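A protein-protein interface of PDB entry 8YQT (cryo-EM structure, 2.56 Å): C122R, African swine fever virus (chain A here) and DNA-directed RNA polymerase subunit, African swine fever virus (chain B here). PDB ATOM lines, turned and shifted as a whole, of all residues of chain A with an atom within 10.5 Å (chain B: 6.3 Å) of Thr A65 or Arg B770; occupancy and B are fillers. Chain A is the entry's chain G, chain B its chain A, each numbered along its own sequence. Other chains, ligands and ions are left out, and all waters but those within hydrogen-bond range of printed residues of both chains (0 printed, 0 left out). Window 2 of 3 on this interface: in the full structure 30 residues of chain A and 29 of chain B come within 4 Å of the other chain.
OD2 of Asp A63 lies within salt-bridge range of NH2 of Arg B777 (3.9 Å).
The backbone NH of Arg B777 is in hydrogen-bond range of the backbone carbonyl oxygen of Thr A65 (2.4 Å).
The side-chain amide oxygen (OD1) of Asn A66 sits at hydrogen-bond distance from the guanidinium group (NH1) of Arg B777, 3.1 Å away.
O of Arg B777 is in hydrogen-bond range of N of Cys A67 (3.1 Å).
The backbone carbonyl oxygen (O) of Phe B778 lies close to the side-chain amide oxygen (OE1) of Gln A83, 3.3 Å away.
The backbone NH (N) of Gln B765 lies within hydrogen-bond range of the backbone carbonyl oxygen (O) of Arg B770, at 3.4 Å.
The backbone carbonyl oxygen (O) of Gly B769 sits at hydrogen-bond distance from the backbone NH (N) of Phe B778 (3.1 Å).
The guanidinium group (NH2) of Arg B770 is in hydrogen-bond range of the backbone carbonyl oxygen (O) of Val B773 (3.1 Å).
NH2 of Arg B770 lies within hydrogen-bond range of O of Tyr B775 (3.0 Å).
ND2 of Asn A66 sits at hydrogen-bond distance from O of Ala A60 (2.8 Å).
O of Cys A67 sits at hydrogen-bond distance from N of Gln A83, 2.9 Å away.
Phe A56 touches Phe B768.
CZ of Phe A56 touches CD of Arg B777, 3.8 Å away.
Phe A56 touches Phe B778.
Thr A65 touches Arg B770 (CG2 to NH1, 3.6 Å).
O of Thr A65 touches CA of Pro B776, 3.2 Å away.
C of Asn A66 touches CB of Pro B776, 3.9 Å away.
Cys A67 touches Pro B776.
Phe B778 touches Cys A67 (O to CB, 3.8 Å).
CA of Ile A84 touches CD2 of Phe B778 (3.6 Å).
Phe B778 touches Cys A85.
Of chain B, only Arg B770, Pro B776 and Arg B777 come within 4 Å of Thr A65.
Of the printed residues of chain A, Arg B770 touches Thr A65.
No residue of chain A comes within 4 Å of Pro B764.
No residue of chain A comes within 4 Å of Phe B766.
No residue of chain A comes within 4 Å of Gly B769.
No residue of chain A comes within 4 Å of Thr B771.
No residue of chain A comes within 4 Å of Val B773.
Of chain A, only Thr A65 (3.2 Å), Asn A66 (3.9 Å) and Cys A67 (3.9 Å) come within 4 Å of Pro B776.
Arg B777 touches just these residues of chain A: Phe A56 (3.8 Å), Asp A63 (2.4 Å), Thr A65 (2.4 Å), Asn A66 (3.1 Å) and Cys A67 (3.1 Å).
Of the printed residues of chain B, Ile A84 touches Phe B778 (3.6 Å).
Printed residues of chain B within 4 Å of Gln A83: Phe B778 (3.3 Å).
Leu B772 touches none of the printed residues of chain A.
Tyr B774 touches none of the printed residues of chain A.
The nearest residue of chain A that does not touch Arg B770 is Asn A66 (6.3 Å).
Along chain A the printed residues that touch a printed residue of chain B span positions 56 to 85.
Printed residues of chain B that touch a printed residue of chain A: Phe B768, Arg B770, Pro B776, Arg B777 and Phe B778.
Hydrophobic or aromatic side chains of chain B that line the printed part of chain A: Phe B768, Pro B776 and Phe B778.
Among the printed residues, 15 pairs touch across the chains.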
ATOM      1  N   PHE A  56       0.529  29.445  24.400  1.00  0.00           N
ATOM      2  CA  PHE A  56       0.628  28.014  24.138  1.00  0.00           C
ATOM      3  C   PHE A  56      -0.657  27.469  23.532  1.00  0.00           C
ATOM      4  O   PHE A  56      -0.611  26.689  22.578  1.00  0.00           O
ATOM      5  CB  PHE A  56       0.970  27.263  25.423  1.00  0.00           C
ATOM      6  CG  PHE A  56       0.980  25.774  25.261  1.00  0.00           C
ATOM      7  CD1 PHE A  56       2.067  25.137  24.693  1.00  0.00           C
ATOM      8  CD2 PHE A  56      -0.103  25.013  25.663  1.00  0.00           C
ATOM      9  CE1 PHE A  56       2.076  23.770  24.534  1.00  0.00           C
ATOM     10  CE2 PHE A  56      -0.099  23.647  25.505  1.00  0.00           C
ATOM     11  CZ  PHE A  56       0.993  23.025  24.940  1.00  0.00           C
ATOM     12  N   ASN A  59      -0.923  28.564  19.948  1.00  0.00           N
ATOM     13  CA  ASN A  59       0.003  27.858  19.071  1.00  0.00           C
ATOM     14  C   ASN A  59      -0.232  26.354  19.010  1.00  0.00           C
ATOM     15  O   ASN A  59       0.373  25.689  18.166  1.00  0.00           O
ATOM     16  CB  ASN A  59       1.448  28.104  19.515  1.00  0.00           C
ATOM     17  CG  ASN A  59       1.952  29.473  19.130  1.00  0.00           C
ATOM     18  OD1 ASN A  59       1.594  30.007  18.082  1.00  0.00           O
ATOM     19  ND2 ASN A  59       2.800  30.044  19.971  1.00  0.00           N
ATOM     20  N   ALA A  60      -1.077  25.810  19.885  1.00  0.00           N
ATOM     21  CA  ALA A  60      -1.239  24.362  19.986  1.00  0.00           C
ATOM     22  C   ALA A  60      -1.567  23.653  18.676  1.00  0.00           C
ATOM     23  O   ALA A  60      -0.945  22.611  18.409  1.00  0.00           O
ATOM     24  CB  ALA A  60      -2.305  24.045  21.045  1.00  0.00           C
ATOM     25  N   PRO A  61      -2.498  24.117  17.834  1.00  0.00           N
ATOM     26  CA  PRO A  61      -2.791  23.372  16.600  1.00  0.00           C
ATOM     27  C   PRO A  61      -1.630  23.308  15.627  1.00  0.00           C
ATOM     28  O   PRO A  61      -1.645  22.452  14.736  1.00  0.00           O
ATOM     29  CB  PRO A  61      -3.970  24.143  15.997  1.00  0.00           C
ATOM     30  CG  PRO A  61      -4.543  24.907  17.125  1.00  0.00           C
ATOM     31  CD  PRO A  61      -3.380  25.287  17.962  1.00  0.00           C
ATOM     32  N   PHE A  62      -0.633  24.179  15.761  1.00  0.00           N
ATOM     33  CA  PHE A  62       0.475  24.232  14.822  1.00  0.00           C
ATOM     34  C   PHE A  62       1.709  23.488  15.306  1.00  0.00           C
ATOM     35  O   PHE A  62       2.580  23.169  14.493  1.00  0.00           O
ATOM     36  CB  PHE A  62       0.837  25.689  14.526  1.00  0.00           C
ATOM     37  CG  PHE A  62      -0.317  26.501  14.036  1.00  0.00           C
ATOM     38  CD1 PHE A  62      -0.720  26.427  12.718  1.00  0.00           C
ATOM     39  CD2 PHE A  62      -1.018  27.319  14.898  1.00  0.00           C
ATOM     40  CE1 PHE A  62      -1.788  27.166  12.266  1.00  0.00           C
ATOM     41  CE2 PHE A  62      -2.089  28.058  14.452  1.00  0.00           C
ATOM     42  CZ  PHE A  62      -2.474  27.981  13.133  1.00  0.00           C
ATOM     43  N   ASP A  63       1.802  23.212  16.592  1.00  0.00           N
ATOM     44  CA  ASP A  63       2.905  22.424  17.117  1.00  0.00           C
ATOM     45  C   ASP A  63       2.702  20.967  16.730  1.00  0.00           C
ATOM     46  O   ASP A  63       1.689  20.369  17.115  1.00  0.00           O
ATOM     47  CB  ASP A  63       2.971  22.578  18.632  1.00  0.00           C
ATOM     48  CG  ASP A  63       4.270  22.075  19.219  1.00  0.00           C
ATOM     49  OD1 ASP A  63       5.177  21.709  18.446  1.00  0.00           O
ATOM     50  OD2 ASP A  63       4.379  22.045  20.460  1.00  0.00           O
ATOM     51  N   PRO A  64       3.617  20.355  15.978  1.00  0.00           N
ATOM     52  CA  PRO A  64       3.443  18.958  15.574  1.00  0.00           C
ATOM     53  C   PRO A  64       3.766  17.939  16.655  1.00  0.00           C
ATOM     54  O   PRO A  64       3.696  16.739  16.383  1.00  0.00           O
ATOM     55  CB  PRO A  64       4.420  18.829  14.397  1.00  0.00           C
ATOM     56  CG  PRO A  64       5.485  19.793  14.703  1.00  0.00           C
ATOM     57  CD  PRO A  64       4.825  20.953  15.385  1.00  0.00           C
ATOM     58  N   THR A  65       4.118  18.375  17.861  1.00  0.00           N
ATOM     59  CA  THR A  65       4.421  17.476  18.963  1.00  0.00           C
ATOM     60  C   THR A  65       3.256  17.317  19.927  1.00  0.00           C
ATOM     61  O   THR A  65       3.417  16.691  20.977  1.00  0.00           O
ATOM     62  CB  THR A  65       5.656  17.963  19.721  1.00  0.00           C
ATOM     63  OG1 THR A  65       5.329  19.144  20.461  1.00  0.00           O
ATOM     64  CG2 THR A  65       6.774  18.280  18.756  1.00  0.00           C
ATOM     65  N   ASN A  66       2.093  17.865  19.600  1.00  0.00           N
ATOM     66  CA  ASN A  66       0.934  17.788  20.473  1.00  0.00           C
ATOM     67  C   ASN A  66       0.077  16.576  20.129  1.00  0.00           C
ATOM     68  O   ASN A  66       0.029  16.119  18.985  1.00  0.00           O
ATOM     69  CB  ASN A  66       0.097  19.060  20.373  1.00  0.00           C
ATOM     70  CG  ASN A  66       0.756  20.240  21.037  1.00  0.00           C
ATOM     71  OD1 ASN A  66       1.458  20.093  22.034  1.00  0.00           O
ATOM     72  ND2 ASN A  66       0.529  21.424  20.494  1.00  0.00           N
ATOM     73  N   CYS A  67      -0.607  16.060  21.145  1.00  0.00           N
ATOM     74  CA  CYS A  67      -1.477  14.910  20.953  1.00  0.00           C
ATOM     75  C   CYS A  67      -2.688  15.296  20.116  1.00  0.00           C
ATOM     76  O   CYS A  67      -3.333  16.316  20.371  1.00  0.00           O
ATOM     77  CB  CYS A  67      -1.921  14.357  22.305  1.00  0.00           C
ATOM     78  SG  CYS A  67      -2.989  12.910  22.224  1.00  0.00           S
ATOM     79  N   GLN A  68      -2.995  14.481  19.119  1.00  0.00           N
ATOM     80  CA  GLN A  68      -4.177  14.663  18.293  1.00  0.00           C
ATOM     81  C   GLN A  68      -5.233  13.636  18.671  1.00  0.00           C
ATOM     82  O   GLN A  68      -4.929  12.544  19.152  1.00  0.00           O
ATOM     83  CB  GLN A  68      -3.828  14.540  16.809  1.00  0.00           C
ATOM     84  CG  GLN A  68      -2.598  15.321  16.401  1.00  0.00           C
ATOM     85  CD  GLN A  68      -2.877  16.791  16.219  1.00  0.00           C
ATOM     86  OE1 GLN A  68      -3.790  17.173  15.495  1.00  0.00           O
ATOM     87  NE2 GLN A  68      -2.092  17.628  16.881  1.00  0.00           N
ATOM     88  N   ILE A  69      -6.489  14.002  18.449  1.00  0.00           N
ATOM     89  CA  ILE A  69      -7.626  13.167  18.805  1.00  0.00           C
ATOM     90  C   ILE A  69      -8.546  13.063  17.597  1.00  0.00           C
ATOM     91  O   ILE A  69      -8.653  14.003  16.802  1.00  0.00           O
ATOM     92  CB  ILE A  69      -8.372  13.726  20.041  1.00  0.00           C
ATOM     93  CG1 ILE A  69      -9.392  12.722  20.566  1.00  0.00           C
ATOM     94  CG2 ILE A  69      -9.040  15.052  19.730  1.00  0.00           C
ATOM     95  CD1 ILE A  69     -10.317  13.294  21.606  1.00  0.00           C
ATOM     96  N   LEU A  81      -8.726  16.860  16.021  1.00  0.00           N
ATOM     97  CA  LEU A  81      -8.511  18.001  16.897  1.00  0.00           C
ATOM     98  C   LEU A  81      -7.223  17.803  17.681  1.00  0.00           C
ATOM     99  O   LEU A  81      -6.681  16.701  17.760  1.00  0.00           O
ATOM    100  CB  LEU A  81      -9.679  18.203  17.868  1.00  0.00           C
ATOM    101  CG  LEU A  81     -11.021  18.651  17.292  1.00  0.00           C
ATOM    102  CD1 LEU A  81     -12.096  18.559  18.356  1.00  0.00           C
ATOM    103  CD2 LEU A  81     -10.932  20.059  16.744  1.00  0.00           C
ATOM    104  N   THR A  82      -6.735  18.893  18.261  1.00  0.00           N
ATOM    105  CA  THR A  82      -5.561  18.860  19.120  1.00  0.00           C
ATOM    106  C   THR A  82      -6.010  18.859  20.573  1.00  0.00           C
ATOM    107  O   THR A  82      -6.744  19.753  21.000  1.00  0.00           O
ATOM    108  CB  THR A  82      -4.648  20.054  18.844  1.00  0.00           C
ATOM    109  OG1 THR A  82      -4.260  20.052  17.468  1.00  0.00           O
ATOM    110  CG2 THR A  82      -3.407  19.983  19.708  1.00  0.00           C
ATOM    111  N   GLN A  83      -5.572  17.856  21.324  1.00  0.00           N
ATOM    112  CA  GLN A  83      -5.972  17.678  22.712  1.00  0.00           C
ATOM    113  C   GLN A  83      -4.816  18.084  23.616  1.00  0.00           C
ATOM    114  O   GLN A  83      -3.709  17.552  23.488  1.00  0.00           O
ATOM    115  CB  GLN A  83      -6.382  16.226  22.968  1.00  0.00           C
ATOM    116  CG  GLN A  83      -6.613  15.863  24.427  1.00  0.00           C
ATOM    117  CD  GLN A  83      -5.368  15.315  25.106  1.00  0.00           C
ATOM    118  OE1 GLN A  83      -4.520  14.694  24.467  1.00  0.00           O
ATOM    119  NE2 GLN A  83      -5.257  15.542  26.408  1.00  0.00           N
ATOM    120  N   ILE A  84      -5.068  19.025  24.523  1.00  0.00           N
ATOM    121  CA  ILE A  84      -4.063  19.447  25.489  1.00  0.00           C
ATOM    122  C   ILE A  84      -4.643  19.312  26.888  1.00  0.00           C
ATOM    123  O   ILE A  84      -5.854  19.420  27.095  1.00  0.00           O
ATOM    124  CB  ILE A  84      -3.565  20.888  25.232  1.00  0.00           C
ATOM    125  CG1 ILE A  84      -4.709  21.891  25.347  1.00  0.00           C
ATOM    126  CG2 ILE A  84      -2.911  20.999  23.865  1.00  0.00           C
ATOM    127  CD1 ILE A  84      -4.264  23.316  25.190  1.00  0.00           C
ATOM    128  N   CYS A  85      -3.763  19.066  27.855  1.00  0.00           N
ATOM    129  CA  CYS A  85      -4.156  18.799  29.237  1.00  0.00           C
ATOM    130  C   CYS A  85      -3.323  19.696  30.148  1.00  0.00           C
ATOM    131  O   CYS A  85      -2.120  19.474  30.316  1.00  0.00           O
ATOM    132  CB  CYS A  85      -3.966  17.326  29.579  1.00  0.00           C
ATOM    133  SG  CYS A  85      -4.539  16.843  31.210  1.00  0.00           S
ATOM    134  N   ARG A  97      -6.991  24.222  14.112  1.00  0.00           N
ATOM    135  CA  ARG A  97      -6.223  25.191  13.339  1.00  0.00           C
ATOM    136  C   ARG A  97      -7.083  26.360  12.885  1.00  0.00           C
ATOM    137  O   ARG A  97      -6.571  27.471  12.711  1.00  0.00           O
ATOM    138  CB  ARG A  97      -5.593  24.502  12.131  1.00  0.00           C
ATOM    139  CG  ARG A  97      -4.075  24.521  12.112  1.00  0.00           C
ATOM    140  CD  ARG A  97      -3.536  23.445  11.182  1.00  0.00           C
ATOM    141  NE  ARG A  97      -2.144  23.118  11.459  1.00  0.00           N
ATOM    142  CZ  ARG A  97      -1.113  23.584  10.767  1.00  0.00           C
ATOM    143  NH1 ARG A  97      -1.282  24.401   9.742  1.00  0.00           N
ATOM    144  NH2 ARG A  97       0.118  23.216  11.110  1.00  0.00           N
ATOM    145  N   GLN B 763       7.776  10.438  34.792  1.00  0.00           N
ATOM    146  CA  GLN B 763       7.385  11.838  34.845  1.00  0.00           C
ATOM    147  C   GLN B 763       7.706  12.526  33.521  1.00  0.00           C
ATOM    148  O   GLN B 763       8.717  12.211  32.889  1.00  0.00           O
ATOM    149  CB  GLN B 763       8.103  12.553  35.984  1.00  0.00           C
ATOM    150  CG  GLN B 763       7.787  12.000  37.358  1.00  0.00           C
ATOM    151  CD  GLN B 763       6.308  12.025  37.661  1.00  0.00           C
ATOM    152  OE1 GLN B 763       5.675  10.983  37.809  1.00  0.00           O
ATOM    153  NE2 GLN B 763       5.745  13.222  37.748  1.00  0.00           N
ATOM    154  N   PRO B 764       6.876  13.465  33.080  1.00  0.00           N
ATOM    155  CA  PRO B 764       7.193  14.181  31.842  1.00  0.00           C
ATOM    156  C   PRO B 764       8.368  15.121  32.043  1.00  0.00           C
ATOM    157  O   PRO B 764       8.239  16.206  32.618  1.00  0.00           O
ATOM    158  CB  PRO B 764       5.898  14.934  31.526  1.00  0.00           C
ATOM    159  CG  PRO B 764       5.196  15.041  32.823  1.00  0.00           C
ATOM    160  CD  PRO B 764       5.546  13.818  33.600  1.00  0.00           C
ATOM    161  N   GLN B 765       9.523  14.698  31.544  1.00  0.00           N
ATOM    162  CA  GLN B 765      10.789  15.384  31.737  1.00  0.00           C
ATOM    163  C   GLN B 765      11.358  15.927  30.436  1.00  0.00           C
ATOM    164  O   GLN B 765      12.271  16.757  30.469  1.00  0.00           O
ATOM    165  CB  GLN B 765      11.784  14.419  32.406  1.00  0.00           C
ATOM    166  CG  GLN B 765      13.254  14.788  32.396  1.00  0.00           C
ATOM    167  CD  GLN B 765      14.099  13.785  33.156  1.00  0.00           C
ATOM    168  OE1 GLN B 765      14.537  12.777  32.601  1.00  0.00           O
ATOM    169  NE2 GLN B 765      14.332  14.055  34.431  1.00  0.00           N
ATOM    170  N   PHE B 766      10.801  15.514  29.300  1.00  0.00           N
ATOM    171  CA  PHE B 766      11.219  15.983  27.984  1.00  0.00           C
ATOM    172  C   PHE B 766      10.270  17.097  27.550  1.00  0.00           C
ATOM    173  O   PHE B 766       9.307  16.881  26.820  1.00  0.00           O
ATOM    174  CB  PHE B 766      11.226  14.819  26.996  1.00  0.00           C
ATOM    175  CG  PHE B 766      11.803  15.152  25.653  1.00  0.00           C
ATOM    176  CD1 PHE B 766      13.158  15.053  25.425  1.00  0.00           C
ATOM    177  CD2 PHE B 766      10.985  15.547  24.613  1.00  0.00           C
ATOM    178  CE1 PHE B 766      13.688  15.350  24.192  1.00  0.00           C
ATOM    179  CE2 PHE B 766      11.511  15.848  23.381  1.00  0.00           C
ATOM    180  CZ  PHE B 766      12.863  15.749  23.170  1.00  0.00           C
ATOM    181  N   SER B 767      10.554  18.312  28.015  1.00  0.00           N
ATOM    182  CA  SER B 767       9.921  19.532  27.508  1.00  0.00           C
ATOM    183  C   SER B 767       8.401  19.540  27.718  1.00  0.00           C
ATOM    184  O   SER B 767       7.615  19.479  26.773  1.00  0.00           O
ATOM    185  CB  SER B 767      10.250  19.734  26.025  1.00  0.00           C
ATOM    186  OG  SER B 767       9.388  18.962  25.208  1.00  0.00           O
ATOM    187  N   PHE B 768       8.010  19.625  28.991  1.00  0.00           N
ATOM    188  CA  PHE B 768       6.663  20.076  29.351  1.00  0.00           C
ATOM    189  C   PHE B 768       5.546  19.207  28.778  1.00  0.00           C
ATOM    190  O   PHE B 768       4.886  19.583  27.805  1.00  0.00           O
ATOM    191  CB  PHE B 768       6.451  21.538  28.936  1.00  0.00           C
ATOM    192  CG  PHE B 768       5.033  22.014  29.111  1.00  0.00           C
ATOM    193  CD1 PHE B 768       4.391  21.885  30.330  1.00  0.00           C
ATOM    194  CD2 PHE B 768       4.334  22.560  28.050  1.00  0.00           C
ATOM    195  CE1 PHE B 768       3.087  22.300  30.490  1.00  0.00           C
ATOM    196  CE2 PHE B 768       3.029  22.978  28.205  1.00  0.00           C
ATOM    197  CZ  PHE B 768       2.406  22.849  29.426  1.00  0.00           C
ATOM    198  N   GLY B 769       5.376  18.010  29.319  1.00  0.00           N
ATOM    199  CA  GLY B 769       4.271  17.165  28.933  1.00  0.00           C
ATOM    200  C   GLY B 769       4.652  15.998  28.061  1.00  0.00           C
ATOM    201  O   GLY B 769       3.795  15.157  27.775  1.00  0.00           O
ATOM    202  N   ARG B 770       5.903  15.922  27.633  1.00  0.00           N
ATOM    203  CA  ARG B 770       6.413  14.798  26.869  1.00  0.00           C
ATOM    204  C   ARG B 770       7.415  14.035  27.717  1.00  0.00           C
ATOM    205  O   ARG B 770       8.271  14.635  28.373  1.00  0.00           O
ATOM    206  CB  ARG B 770       7.076  15.261  25.573  1.00  0.00           C
ATOM    207  CG  ARG B 770       6.315  16.324  24.826  1.00  0.00           C
ATOM    208  CD  ARG B 770       7.040  16.685  23.560  1.00  0.00           C
ATOM    209  NE  ARG B 770       7.140  15.548  22.658  1.00  0.00           N
ATOM    210  CZ  ARG B 770       7.932  15.503  21.596  1.00  0.00           C
ATOM    211  NH1 ARG B 770       8.722  16.514  21.282  1.00  0.00           N
ATOM    212  NH2 ARG B 770       7.927  14.419  20.831  1.00  0.00           N
ATOM    213  N   THR B 771       7.293  12.713  27.717  1.00  0.00           N
ATOM    214  CA  THR B 771       8.248  11.871  28.420  1.00  0.00           C
ATOM    215  C   THR B 771       9.459  11.538  27.565  1.00  0.00           C
ATOM    216  O   THR B 771      10.563  11.392  28.099  1.00  0.00           O
ATOM    217  CB  THR B 771       7.566  10.585  28.885  1.00  0.00           C
ATOM    218  OG1 THR B 771       6.961   9.935  27.764  1.00  0.00           O
ATOM    219  CG2 THR B 771       6.494  10.899  29.906  1.00  0.00           C
ATOM    220  N   LEU B 772       9.279  11.424  26.252  1.00  0.00           N
ATOM    221  CA  LEU B 772      10.365  11.150  25.326  1.00  0.00           C
ATOM    222  C   LEU B 772      10.068  11.860  24.016  1.00  0.00           C
ATOM    223  O   LEU B 772       8.972  12.383  23.805  1.00  0.00           O
ATOM    224  CB  LEU B 772      10.549   9.646  25.095  1.00  0.00           C
ATOM    225  CG  LEU B 772      11.196   8.778  26.176  1.00  0.00           C
ATOM    226  CD1 LEU B 772      11.195   7.329  25.740  1.00  0.00           C
ATOM    227  CD2 LEU B 772      12.603   9.243  26.490  1.00  0.00           C
ATOM    228  N   VAL B 773      11.062  11.877  23.128  1.00  0.00           N
ATOM    229  CA  VAL B 773      10.870  12.415  21.788  1.00  0.00           C
ATOM    230  C   VAL B 773       9.987  11.525  20.930  1.00  0.00           C
ATOM    231  O   VAL B 773       9.546  11.946  19.856  1.00  0.00           O
ATOM    232  CB  VAL B 773      12.240  12.628  21.111  1.00  0.00           C
ATOM    233  CG1 VAL B 773      12.777  11.318  20.574  1.00  0.00           C
ATOM    234  CG2 VAL B 773      12.145  13.674  20.014  1.00  0.00           C
ATOM    235  N   TYR B 774       9.713  10.305  21.383  1.00  0.00           N
ATOM    236  CA  TYR B 774       8.917   9.359  20.621  1.00  0.00           C
ATOM    237  C   TYR B 774       7.426   9.496  20.867  1.00  0.00           C
ATOM    238  O   TYR B 774       6.634   8.948  20.095  1.00  0.00           O
ATOM    239  CB  TYR B 774       9.360   7.932  20.941  1.00  0.00           C
ATOM    240  CG  TYR B 774      10.815   7.697  20.641  1.00  0.00           C
ATOM    241  CD1 TYR B 774      11.296   7.790  19.346  1.00  0.00           C
ATOM    242  CD2 TYR B 774      11.711   7.394  21.651  1.00  0.00           C
ATOM    243  CE1 TYR B 774      12.623   7.583  19.066  1.00  0.00           C
ATOM    244  CE2 TYR B 774      13.040   7.184  21.378  1.00  0.00           C
ATOM    245  CZ  TYR B 774      13.491   7.280  20.084  1.00  0.00           C
ATOM    246  OH  TYR B 774      14.819   7.075  19.803  1.00  0.00           O
ATOM    247  N   TYR B 775       7.026  10.221  21.904  1.00  0.00           N
ATOM    248  CA  TYR B 775       5.622  10.371  22.216  1.00  0.00           C
ATOM    249  C   TYR B 775       5.224  11.838  22.155  1.00  0.00           C
ATOM    250  O   TYR B 775       6.038  12.717  22.445  1.00  0.00           O
ATOM    251  CB  TYR B 775       5.311   9.806  23.605  1.00  0.00           C
ATOM    252  CG  TYR B 775       5.663   8.348  23.730  1.00  0.00           C
ATOM    253  CD1 TYR B 775       4.887   7.376  23.122  1.00  0.00           C
ATOM    254  CD2 TYR B 775       6.780   7.945  24.443  1.00  0.00           C
ATOM    255  CE1 TYR B 775       5.207   6.050  23.226  1.00  0.00           C
ATOM    256  CE2 TYR B 775       7.106   6.618  24.551  1.00  0.00           C
ATOM    257  CZ  TYR B 775       6.315   5.675  23.941  1.00  0.00           C
ATOM    258  OH  TYR B 775       6.632   4.344  24.046  1.00  0.00           O
ATOM    259  N   PRO B 776       3.990  12.132  21.773  1.00  0.00           N
ATOM    260  CA  PRO B 776       3.549  13.523  21.663  1.00  0.00           C
ATOM    261  C   PRO B 776       3.366  14.147  23.041  1.00  0.00           C
ATOM    262  O   PRO B 776       3.540  13.509  24.074  1.00  0.00           O
ATOM    263  CB  PRO B 776       2.222  13.405  20.911  1.00  0.00           C
ATOM    264  CG  PRO B 776       1.744  12.052  21.209  1.00  0.00           C
ATOM    265  CD  PRO B 776       2.955  11.191  21.323  1.00  0.00           C
ATOM    266  N   ARG B 777       3.025  15.429  23.036  1.00  0.00           N
ATOM    267  CA  ARG B 777       2.778  16.152  24.270  1.00  0.00           C
ATOM    268  C   ARG B 777       1.384  15.833  24.782  1.00  0.00           C
ATOM    269  O   ARG B 777       0.437  15.713  24.001  1.00  0.00           O
ATOM    270  CB  ARG B 777       2.935  17.655  24.042  1.00  0.00           C
ATOM    271  CG  ARG B 777       2.996  18.477  25.308  1.00  0.00           C
ATOM    272  CD  ARG B 777       3.261  19.936  25.008  1.00  0.00           C
ATOM    273  NE  ARG B 777       4.672  20.199  24.763  1.00  0.00           N
ATOM    274  CZ  ARG B 777       5.154  20.697  23.634  1.00  0.00           C
ATOM    275  NH1 ARG B 777       4.365  20.996  22.618  1.00  0.00           N
ATOM    276  NH2 ARG B 777       6.463  20.898  23.522  1.00  0.00           N
ATOM    277  N   PHE B 778       1.266  15.686  26.102  1.00  0.00           N
ATOM    278  CA  PHE B 778       0.009  15.315  26.754  1.00  0.00           C
ATOM    279  C   PHE B 778      -0.526  13.992  26.216  1.00  0.00           C
ATOM    280  O   PHE B 778      -1.732  13.815  26.044  1.00  0.00           O
ATOM    281  CB  PHE B 778      -1.041  16.418  26.616  1.00  0.00           C
ATOM    282  CG  PHE B 778      -0.514  17.790  26.888  1.00  0.00           C
ATOM    283  CD1 PHE B 778       0.039  18.102  28.115  1.00  0.00           C
ATOM    284  CD2 PHE B 778      -0.572  18.769  25.917  1.00  0.00           C
ATOM    285  CE1 PHE B 778       0.525  19.359  28.364  1.00  0.00           C
ATOM    286  CE2 PHE B 778      -0.089  20.027  26.164  1.00  0.00           C
ATOM    287  CZ  PHE B 778       0.461  20.324  27.389  1.00  0.00           C
